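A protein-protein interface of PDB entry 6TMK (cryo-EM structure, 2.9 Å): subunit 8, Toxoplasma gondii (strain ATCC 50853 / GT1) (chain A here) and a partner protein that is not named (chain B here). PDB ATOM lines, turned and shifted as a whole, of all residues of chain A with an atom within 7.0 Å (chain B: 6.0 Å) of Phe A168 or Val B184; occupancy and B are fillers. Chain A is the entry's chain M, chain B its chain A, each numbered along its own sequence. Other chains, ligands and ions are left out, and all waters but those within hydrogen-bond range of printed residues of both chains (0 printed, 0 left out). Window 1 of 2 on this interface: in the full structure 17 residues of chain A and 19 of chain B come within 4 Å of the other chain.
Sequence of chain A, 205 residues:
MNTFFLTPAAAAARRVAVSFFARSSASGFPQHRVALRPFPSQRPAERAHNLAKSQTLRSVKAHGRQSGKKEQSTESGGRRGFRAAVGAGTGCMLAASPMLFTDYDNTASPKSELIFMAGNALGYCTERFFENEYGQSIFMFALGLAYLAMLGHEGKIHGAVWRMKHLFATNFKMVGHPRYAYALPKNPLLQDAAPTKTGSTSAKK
Phe A168 touches just these residues of chain B: Trp B166 (3.6 Å) and Val B184 (3.5 Å).
Of chain A, only Met A164, Leu A167 and Phe A168 come within 4 Å of Val B184.
Of the printed residues of chain B, Leu A167 touches Val B184.
Printed residues of chain B within 4 Å of Ala A169: Trp B159.
Printed residues of chain A within 4 Å of Trp B159: Val A161, Met A164, Lys A165 and Ala A169.
Of the printed residues of chain A, Trp B166 touches Phe A168, Met A174 and Gly A176.
Gly A159 touches none of the printed residues of chain B.
The nearest residue of chain B that does not touch Phe A168 is Asp B185 (4.6 Å).
The nearest residue of chain A that does not touch Val B184 is Arg A163 (4.1 Å).
The backbone carbonyl oxygen (O) of Gly A159 sits close to the guanidinium group (NH1) of Arg A163.
Of the 8 printed residues of chain B, 6 touch a printed residue of chain A.
Hydrophobic or aromatic side chains of chain B that line the printed part of chain A: Trp B159, Trp B166, Phe B169 and Val B184.
Of the 18 printed residues of chain A, 10 touch a printed residue of chain B.
Printed residues of chain A that touch a printed residue of chain B: Val A161, Arg A163, Met A164, Lys A165, Leu A167, Phe A168, Ala A169, Met A174, Gly A176 and His A177.
Hydrophobic or aromatic side chains of chain A within 4 Å of the printed part of chain B: Val A161, Met A164, Leu A167, Phe A168, Ala A169, Met A174 and His A177.
Along chain A the printed residues that touch a printed residue of chain B span positions 161 to 177.
Among the printed residues, merely in contact across the chains: Val A161 with Trp B159 (3.8 Å), Arg A163 with Gly B182 (3.7 Å), Met A164 with Trp B159 (3.9 Å), Met A164 with Phe B169 (3.7 Å), Met A164 with Val B184 (3.6 Å), Lys A165 with Trp B159 (3.6 Å), Leu A167 with Val B184 (3.9 Å), Phe A168 with Trp B166 (3.6 Å), Phe A168 with Val B184 (3.5 Å), Ala A169 with Trp B159 (3.6 Å), Met A174 with Trp B166 (3.8 Å), Gly A176 with Trp B166 (3.7 Å) and His A177 with Phe B169 (3.7 Å).
OD1 of Asp B185 sits at hydrogen-bond distance from NE2 of His A177, at 2.8 Å.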
ATOM      1  N   GLY A 159      14.612  -0.127   7.164  1.00  0.00           N
ATOM      2  CA  GLY A 159      13.373  -0.483   7.834  1.00  0.00           C
ATOM      3  C   GLY A 159      13.589  -1.467   8.965  1.00  0.00           C
ATOM      4  O   GLY A 159      12.999  -1.336  10.042  1.00  0.00           O
ATOM      5  N   ALA A 160      14.445  -2.461   8.739  1.00  0.00           N
ATOM      6  CA  ALA A 160      14.715  -3.450   9.773  1.00  0.00           C
ATOM      7  C   ALA A 160      15.295  -2.793  11.016  1.00  0.00           C
ATOM      8  O   ALA A 160      14.854  -3.066  12.137  1.00  0.00           O
ATOM      9  CB  ALA A 160      15.663  -4.518   9.243  1.00  0.00           C
ATOM     10  N   VAL A 161      16.287  -1.922  10.840  1.00  0.00           N
ATOM     11  CA  VAL A 161      16.901  -1.272  11.993  1.00  0.00           C
ATOM     12  C   VAL A 161      15.929  -0.300  12.643  1.00  0.00           C
ATOM     13  O   VAL A 161      15.921  -0.135  13.868  1.00  0.00           O
ATOM     14  CB  VAL A 161      18.202  -0.565  11.575  1.00  0.00           C
ATOM     15  CG1 VAL A 161      18.839   0.107  12.761  1.00  0.00           C
ATOM     16  CG2 VAL A 161      19.162  -1.540  10.976  1.00  0.00           C
ATOM     17  N   ARG A 163      12.762  -0.618  12.915  1.00  0.00           N
ATOM     18  CA  ARG A 163      11.861  -1.383  13.768  1.00  0.00           C
ATOM     19  C   ARG A 163      12.590  -1.974  14.968  1.00  0.00           C
ATOM     20  O   ARG A 163      12.036  -2.022  16.075  1.00  0.00           O
ATOM     21  CB  ARG A 163      11.187  -2.486  12.960  1.00  0.00           C
ATOM     22  CG  ARG A 163      10.282  -1.961  11.881  1.00  0.00           C
ATOM     23  CD  ARG A 163       9.599  -3.051  11.100  1.00  0.00           C
ATOM     24  NE  ARG A 163       8.762  -2.477  10.053  1.00  0.00           N
ATOM     25  CZ  ARG A 163       9.122  -2.350   8.781  1.00  0.00           C
ATOM     26  NH1 ARG A 163      10.304  -2.768   8.365  1.00  0.00           N
ATOM     27  NH2 ARG A 163       8.292  -1.797   7.916  1.00  0.00           N
ATOM     28  N   MET A 164      13.820  -2.446  14.758  1.00  0.00           N
ATOM     29  CA  MET A 164      14.630  -2.957  15.855  1.00  0.00           C
ATOM     30  C   MET A 164      14.762  -1.921  16.952  1.00  0.00           C
ATOM     31  O   MET A 164      14.667  -2.243  18.138  1.00  0.00           O
ATOM     32  CB  MET A 164      16.013  -3.350  15.348  1.00  0.00           C
ATOM     33  CG  MET A 164      16.089  -4.714  14.750  1.00  0.00           C
ATOM     34  SD  MET A 164      17.729  -5.104  14.131  1.00  0.00           S
ATOM     35  CE  MET A 164      17.296  -6.274  12.852  1.00  0.00           C
ATOM     36  N   LYS A 165      14.994  -0.670  16.575  1.00  0.00           N
ATOM     37  CA  LYS A 165      15.099   0.395  17.560  1.00  0.00           C
ATOM     38  C   LYS A 165      13.880   0.405  18.467  1.00  0.00           C
ATOM     39  O   LYS A 165      13.977   0.156  19.675  1.00  0.00           O
ATOM     40  CB  LYS A 165      15.252   1.728  16.836  1.00  0.00           C
ATOM     41  CG  LYS A 165      15.413   2.919  17.719  1.00  0.00           C
ATOM     42  CD  LYS A 165      15.790   4.134  16.910  1.00  0.00           C
ATOM     43  CE  LYS A 165      14.624   4.643  16.110  1.00  0.00           C
ATOM     44  NZ  LYS A 165      14.852   6.007  15.598  1.00  0.00           N
ATOM     45  N   HIS A 166      12.707   0.620  17.877  1.00  0.00           N
ATOM     46  CA  HIS A 166      11.496   0.778  18.664  1.00  0.00           C
ATOM     47  C   HIS A 166      11.179  -0.463  19.480  1.00  0.00           C
ATOM     48  O   HIS A 166      10.663  -0.349  20.597  1.00  0.00           O
ATOM     49  CB  HIS A 166      10.332   1.111  17.740  1.00  0.00           C
ATOM     50  CG  HIS A 166      10.373   2.498  17.188  1.00  0.00           C
ATOM     51  ND1 HIS A 166      10.988   2.806  15.994  1.00  0.00           N
ATOM     52  CD2 HIS A 166       9.859   3.659  17.654  1.00  0.00           C
ATOM     53  CE1 HIS A 166      10.862   4.097  15.758  1.00  0.00           C
ATOM     54  NE2 HIS A 166      10.178   4.638  16.748  1.00  0.00           N
ATOM     55  N   LEU A 167      11.473  -1.654  18.958  1.00  0.00           N
ATOM     56  CA  LEU A 167      11.016  -2.874  19.605  1.00  0.00           C
ATOM     57  C   LEU A 167      12.045  -3.513  20.525  1.00  0.00           C
ATOM     58  O   LEU A 167      11.684  -4.420  21.282  1.00  0.00           O
ATOM     59  CB  LEU A 167      10.598  -3.899  18.552  1.00  0.00           C
ATOM     60  CG  LEU A 167       9.507  -3.477  17.579  1.00  0.00           C
ATOM     61  CD1 LEU A 167       9.140  -4.643  16.723  1.00  0.00           C
ATOM     62  CD2 LEU A 167       8.302  -2.964  18.320  1.00  0.00           C
ATOM     63  N   PHE A 168      13.297  -3.077  20.491  1.00  0.00           N
ATOM     64  CA  PHE A 168      14.340  -3.642  21.331  1.00  0.00           C
ATOM     65  C   PHE A 168      14.970  -2.659  22.297  1.00  0.00           C
ATOM     66  O   PHE A 168      15.463  -3.089  23.341  1.00  0.00           O
ATOM     67  CB  PHE A 168      15.464  -4.234  20.468  1.00  0.00           C
ATOM     68  CG  PHE A 168      15.048  -5.400  19.617  1.00  0.00           C
ATOM     69  CD1 PHE A 168      13.848  -6.045  19.819  1.00  0.00           C
ATOM     70  CD2 PHE A 168      15.875  -5.853  18.614  1.00  0.00           C
ATOM     71  CE1 PHE A 168      13.482  -7.114  19.037  1.00  0.00           C
ATOM     72  CE2 PHE A 168      15.516  -6.920  17.832  1.00  0.00           C
ATOM     73  CZ  PHE A 168      14.320  -7.551  18.044  1.00  0.00           C
ATOM     74  N   ALA A 169      14.984  -1.363  21.994  1.00  0.00           N
ATOM     75  CA  ALA A 169      15.819  -0.444  22.743  1.00  0.00           C
ATOM     76  C   ALA A 169      15.220  -0.033  24.080  1.00  0.00           C
ATOM     77  O   ALA A 169      15.904   0.636  24.861  1.00  0.00           O
ATOM     78  CB  ALA A 169      16.090   0.799  21.899  1.00  0.00           C
ATOM     79  N   THR A 170      13.973  -0.408  24.366  1.00  0.00           N
ATOM     80  CA  THR A 170      13.295   0.045  25.574  1.00  0.00           C
ATOM     81  C   THR A 170      12.552  -1.090  26.265  1.00  0.00           C
ATOM     82  O   THR A 170      11.516  -0.862  26.897  1.00  0.00           O
ATOM     83  CB  THR A 170      12.320   1.170  25.258  1.00  0.00           C
ATOM     84  OG1 THR A 170      11.533   0.809  24.120  1.00  0.00           O
ATOM     85  CG2 THR A 170      13.064   2.435  24.962  1.00  0.00           C
ATOM     86  N   ASN A 171      13.066  -2.312  26.168  1.00  0.00           N
ATOM     87  CA  ASN A 171      12.380  -3.486  26.684  1.00  0.00           C
ATOM     88  C   ASN A 171      12.778  -3.809  28.121  1.00  0.00           C
ATOM     89  O   ASN A 171      11.915  -4.103  28.953  1.00  0.00           O
ATOM     90  CB  ASN A 171      12.647  -4.682  25.777  1.00  0.00           C
ATOM     91  CG  ASN A 171      11.599  -5.756  25.916  1.00  0.00           C
ATOM     92  OD1 ASN A 171      11.191  -6.106  27.022  1.00  0.00           O
ATOM     93  ND2 ASN A 171      11.146  -6.279  24.793  1.00  0.00           N
ATOM     94  N   PHE A 172      14.077  -3.767  28.412  1.00  0.00           N
ATOM     95  CA  PHE A 172      14.672  -4.229  29.666  1.00  0.00           C
ATOM     96  C   PHE A 172      14.695  -5.750  29.747  1.00  0.00           C
ATOM     97  O   PHE A 172      15.295  -6.313  30.667  1.00  0.00           O
ATOM     98  CB  PHE A 172      13.930  -3.687  30.893  1.00  0.00           C
ATOM     99  CG  PHE A 172      13.971  -2.201  31.031  1.00  0.00           C
ATOM    100  CD1 PHE A 172      14.840  -1.609  31.919  1.00  0.00           C
ATOM    101  CD2 PHE A 172      13.120  -1.398  30.302  1.00  0.00           C
ATOM    102  CE1 PHE A 172      14.875  -0.244  32.064  1.00  0.00           C
ATOM    103  CE2 PHE A 172      13.154  -0.035  30.441  1.00  0.00           C
ATOM    104  CZ  PHE A 172      14.033   0.542  31.326  1.00  0.00           C
ATOM    105  N   LYS A 173      14.061  -6.426  28.790  1.00  0.00           N
ATOM    106  CA  LYS A 173      14.072  -7.878  28.735  1.00  0.00           C
ATOM    107  C   LYS A 173      14.969  -8.426  27.643  1.00  0.00           C
ATOM    108  O   LYS A 173      15.330  -9.605  27.699  1.00  0.00           O
ATOM    109  CB  LYS A 173      12.656  -8.418  28.518  1.00  0.00           C
ATOM    110  CG  LYS A 173      11.650  -7.913  29.521  1.00  0.00           C
ATOM    111  CD  LYS A 173      10.251  -8.431  29.229  1.00  0.00           C
ATOM    112  CE  LYS A 173      10.191  -9.951  29.227  1.00  0.00           C
ATOM    113  NZ  LYS A 173      10.957 -10.570  30.342  1.00  0.00           N
ATOM    114  N   MET A 174      15.331  -7.609  26.661  1.00  0.00           N
ATOM    115  CA  MET A 174      16.181  -8.020  25.555  1.00  0.00           C
ATOM    116  C   MET A 174      17.521  -7.317  25.733  1.00  0.00           C
ATOM    117  O   MET A 174      17.783  -6.274  25.135  1.00  0.00           O
ATOM    118  CB  MET A 174      15.542  -7.687  24.206  1.00  0.00           C
ATOM    119  CG  MET A 174      14.220  -8.375  23.956  1.00  0.00           C
ATOM    120  SD  MET A 174      13.690  -8.264  22.244  1.00  0.00           S
ATOM    121  CE  MET A 174      14.870  -9.366  21.474  1.00  0.00           C
ATOM    122  N   VAL A 175      18.379  -7.904  26.567  1.00  0.00           N
ATOM    123  CA  VAL A 175      19.766  -7.466  26.580  1.00  0.00           C
ATOM    124  C   VAL A 175      20.474  -7.995  25.347  1.00  0.00           C
ATOM    125  O   VAL A 175      21.387  -7.353  24.815  1.00  0.00           O
ATOM    126  CB  VAL A 175      20.460  -7.923  27.874  1.00  0.00           C
ATOM    127  CG1 VAL A 175      19.643  -7.534  29.066  1.00  0.00           C
ATOM    128  CG2 VAL A 175      20.654  -9.408  27.864  1.00  0.00           C
ATOM    129  N   GLY A 176      20.068  -9.160  24.876  1.00  0.00           N
ATOM    130  CA  GLY A 176      20.461  -9.654  23.571  1.00  0.00           C
ATOM    131  C   GLY A 176      19.328 -10.442  22.970  1.00  0.00           C
ATOM    132  O   GLY A 176      18.158 -10.216  23.295  1.00  0.00           O
ATOM    133  N   HIS A 177      19.662 -11.352  22.126  1.00  0.00           N
ATOM    134  CA  HIS A 177      18.628 -12.174  21.531  1.00  0.00           C
ATOM    135  C   HIS A 177      18.355 -13.388  22.415  1.00  0.00           C
ATOM    136  O   HIS A 177      19.272 -13.916  23.048  1.00  0.00           O
ATOM    137  CB  HIS A 177      19.043 -12.628  20.139  1.00  0.00           C
ATOM    138  CG  HIS A 177      17.910 -13.150  19.318  1.00  0.00           C
ATOM    139  ND1 HIS A 177      17.714 -14.494  19.089  1.00  0.00           N
ATOM    140  CD2 HIS A 177      16.902 -12.510  18.683  1.00  0.00           C
ATOM    141  CE1 HIS A 177      16.636 -14.657  18.344  1.00  0.00           C
ATOM    142  NE2 HIS A 177      16.125 -13.469  18.084  1.00  0.00           N
ATOM    143  N   TRP B 159      21.772   5.599  17.149  1.00  0.00           N
ATOM    144  CA  TRP B 159      21.439   4.500  18.043  1.00  0.00           C
ATOM    145  C   TRP B 159      22.270   3.265  17.739  1.00  0.00           C
ATOM    146  O   TRP B 159      22.772   2.602  18.654  1.00  0.00           O
ATOM    147  CB  TRP B 159      19.951   4.175  17.945  1.00  0.00           C
ATOM    148  CG  TRP B 159      19.600   2.932  18.666  1.00  0.00           C
ATOM    149  CD1 TRP B 159      19.575   2.756  20.006  1.00  0.00           C
ATOM    150  CD2 TRP B 159      19.234   1.677  18.089  1.00  0.00           C
ATOM    151  NE1 TRP B 159      19.216   1.471  20.309  1.00  0.00           N
ATOM    152  CE2 TRP B 159      19.001   0.787  19.145  1.00  0.00           C
ATOM    153  CE3 TRP B 159      19.079   1.221  16.780  1.00  0.00           C
ATOM    154  CZ2 TRP B 159      18.622  -0.529  18.937  1.00  0.00           C
ATOM    155  CZ3 TRP B 159      18.706  -0.080  16.581  1.00  0.00           C
ATOM    156  CH2 TRP B 159      18.480  -0.941  17.650  1.00  0.00           C
ATOM    157  N   TRP B 166      23.399  -5.130  18.674  1.00  0.00           N
ATOM    158  CA  TRP B 166      22.483  -5.246  17.554  1.00  0.00           C
ATOM    159  C   TRP B 166      23.152  -4.881  16.240  1.00  0.00           C
ATOM    160  O   TRP B 166      22.607  -5.184  15.175  1.00  0.00           O
ATOM    161  CB  TRP B 166      21.260  -4.369  17.797  1.00  0.00           C
ATOM    162  CG  TRP B 166      20.513  -4.740  19.028  1.00  0.00           C
ATOM    163  CD1 TRP B 166      20.390  -4.001  20.157  1.00  0.00           C
ATOM    164  CD2 TRP B 166      19.794  -5.954  19.265  1.00  0.00           C
ATOM    165  NE1 TRP B 166      19.638  -4.669  21.083  1.00  0.00           N
ATOM    166  CE2 TRP B 166      19.258  -5.873  20.559  1.00  0.00           C
ATOM    167  CE3 TRP B 166      19.549  -7.098  18.508  1.00  0.00           C
ATOM    168  CZ2 TRP B 166      18.497  -6.887  21.110  1.00  0.00           C
ATOM    169  CZ3 TRP B 166      18.792  -8.102  19.060  1.00  0.00           C
ATOM    170  CH2 TRP B 166      18.273  -7.991  20.345  1.00  0.00           C
ATOM    171  N   PHE B 169      23.888  -8.218  15.101  1.00  0.00           N
ATOM    172  CA  PHE B 169      22.660  -8.858  14.656  1.00  0.00           C
ATOM    173  C   PHE B 169      22.330  -8.468  13.221  1.00  0.00           C
ATOM    174  O   PHE B 169      21.829  -9.289  12.445  1.00  0.00           O
ATOM    175  CB  PHE B 169      21.539  -8.487  15.618  1.00  0.00           C
ATOM    176  CG  PHE B 169      20.309  -9.317  15.475  1.00  0.00           C
ATOM    177  CD1 PHE B 169      20.244 -10.575  16.031  1.00  0.00           C
ATOM    178  CD2 PHE B 169      19.204  -8.830  14.819  1.00  0.00           C
ATOM    179  CE1 PHE B 169      19.117 -11.333  15.909  1.00  0.00           C
ATOM    180  CE2 PHE B 169      18.075  -9.587  14.698  1.00  0.00           C
ATOM    181  CZ  PHE B 169      18.028 -10.836  15.249  1.00  0.00           C
ATOM    182  N   GLY B 182      13.346  -8.320   5.623  1.00  0.00           N
ATOM    183  CA  GLY B 182      13.545  -7.119   6.402  1.00  0.00           C
ATOM    184  C   GLY B 182      12.600  -7.027   7.574  1.00  0.00           C
ATOM    185  O   GLY B 182      11.847  -6.058   7.702  1.00  0.00           O
ATOM    186  N   VAL B 183      12.639  -8.027   8.445  1.00  0.00           N
ATOM    187  CA  VAL B 183      11.795  -8.055   9.625  1.00  0.00           C
ATOM    188  C   VAL B 183      12.681  -7.853  10.844  1.00  0.00           C
ATOM    189  O   VAL B 183      13.902  -8.024  10.800  1.00  0.00           O
ATOM    190  CB  VAL B 183      10.981  -9.360   9.737  1.00  0.00           C
ATOM    191  CG1 VAL B 183       9.995  -9.456   8.604  1.00  0.00           C
ATOM    192  CG2 VAL B 183      11.890 -10.568   9.745  1.00  0.00           C
ATOM    193  N   VAL B 184      12.043  -7.479  11.951  1.00  0.00           N
ATOM    194  CA  VAL B 184      12.793  -7.138  13.151  1.00  0.00           C
ATOM    195  C   VAL B 184      13.533  -8.350  13.703  1.00  0.00           C
ATOM    196  O   VAL B 184      14.635  -8.216  14.246  1.00  0.00           O
ATOM    197  CB  VAL B 184      11.848  -6.530  14.199  1.00  0.00           C
ATOM    198  CG1 VAL B 184      10.771  -7.522  14.586  1.00  0.00           C
ATOM    199  CG2 VAL B 184      12.622  -6.074  15.402  1.00  0.00           C
ATOM    200  N   ASP B 185      12.954  -9.543  13.575  1.00  0.00           N
ATOM    201  CA  ASP B 185      13.517 -10.764  14.148  1.00  0.00           C
ATOM    202  C   ASP B 185      13.475 -11.869  13.103  1.00  0.00           C
ATOM    203  O   ASP B 185      12.483 -12.601  12.992  1.00  0.00           O
ATOM    204  CB  ASP B 185      12.767 -11.175  15.411  1.00  0.00           C
ATOM    205  CG  ASP B 185      13.620 -12.000  16.347  1.00  0.00           C
ATOM    206  OD1 ASP B 185      14.603 -12.607  15.877  1.00  0.00           O
ATOM    207  OD2 ASP B 185      13.308 -12.044  17.556  1.00  0.00           O
ATOM    208  N   PRO B 186      14.539 -12.015  12.308  1.00  0.00           N
ATOM    209  CA  PRO B 186      14.597 -13.114  11.337  1.00  0.00           C
ATOM    210  C   PRO B 186      14.921 -14.466  11.945  1.00  0.00           C
ATOM    211  O   PRO B 186      14.735 -15.485  11.266  1.00  0.00           O
ATOM    212  CB  PRO B 186      15.709 -12.673  10.378  1.00  0.00           C
ATOM    213  CG  PRO B 186      15.989 -11.268  10.691  1.00  0.00           C
ATOM    214  CD  PRO B 186      15.627 -11.056  12.105  1.00  0.00           C
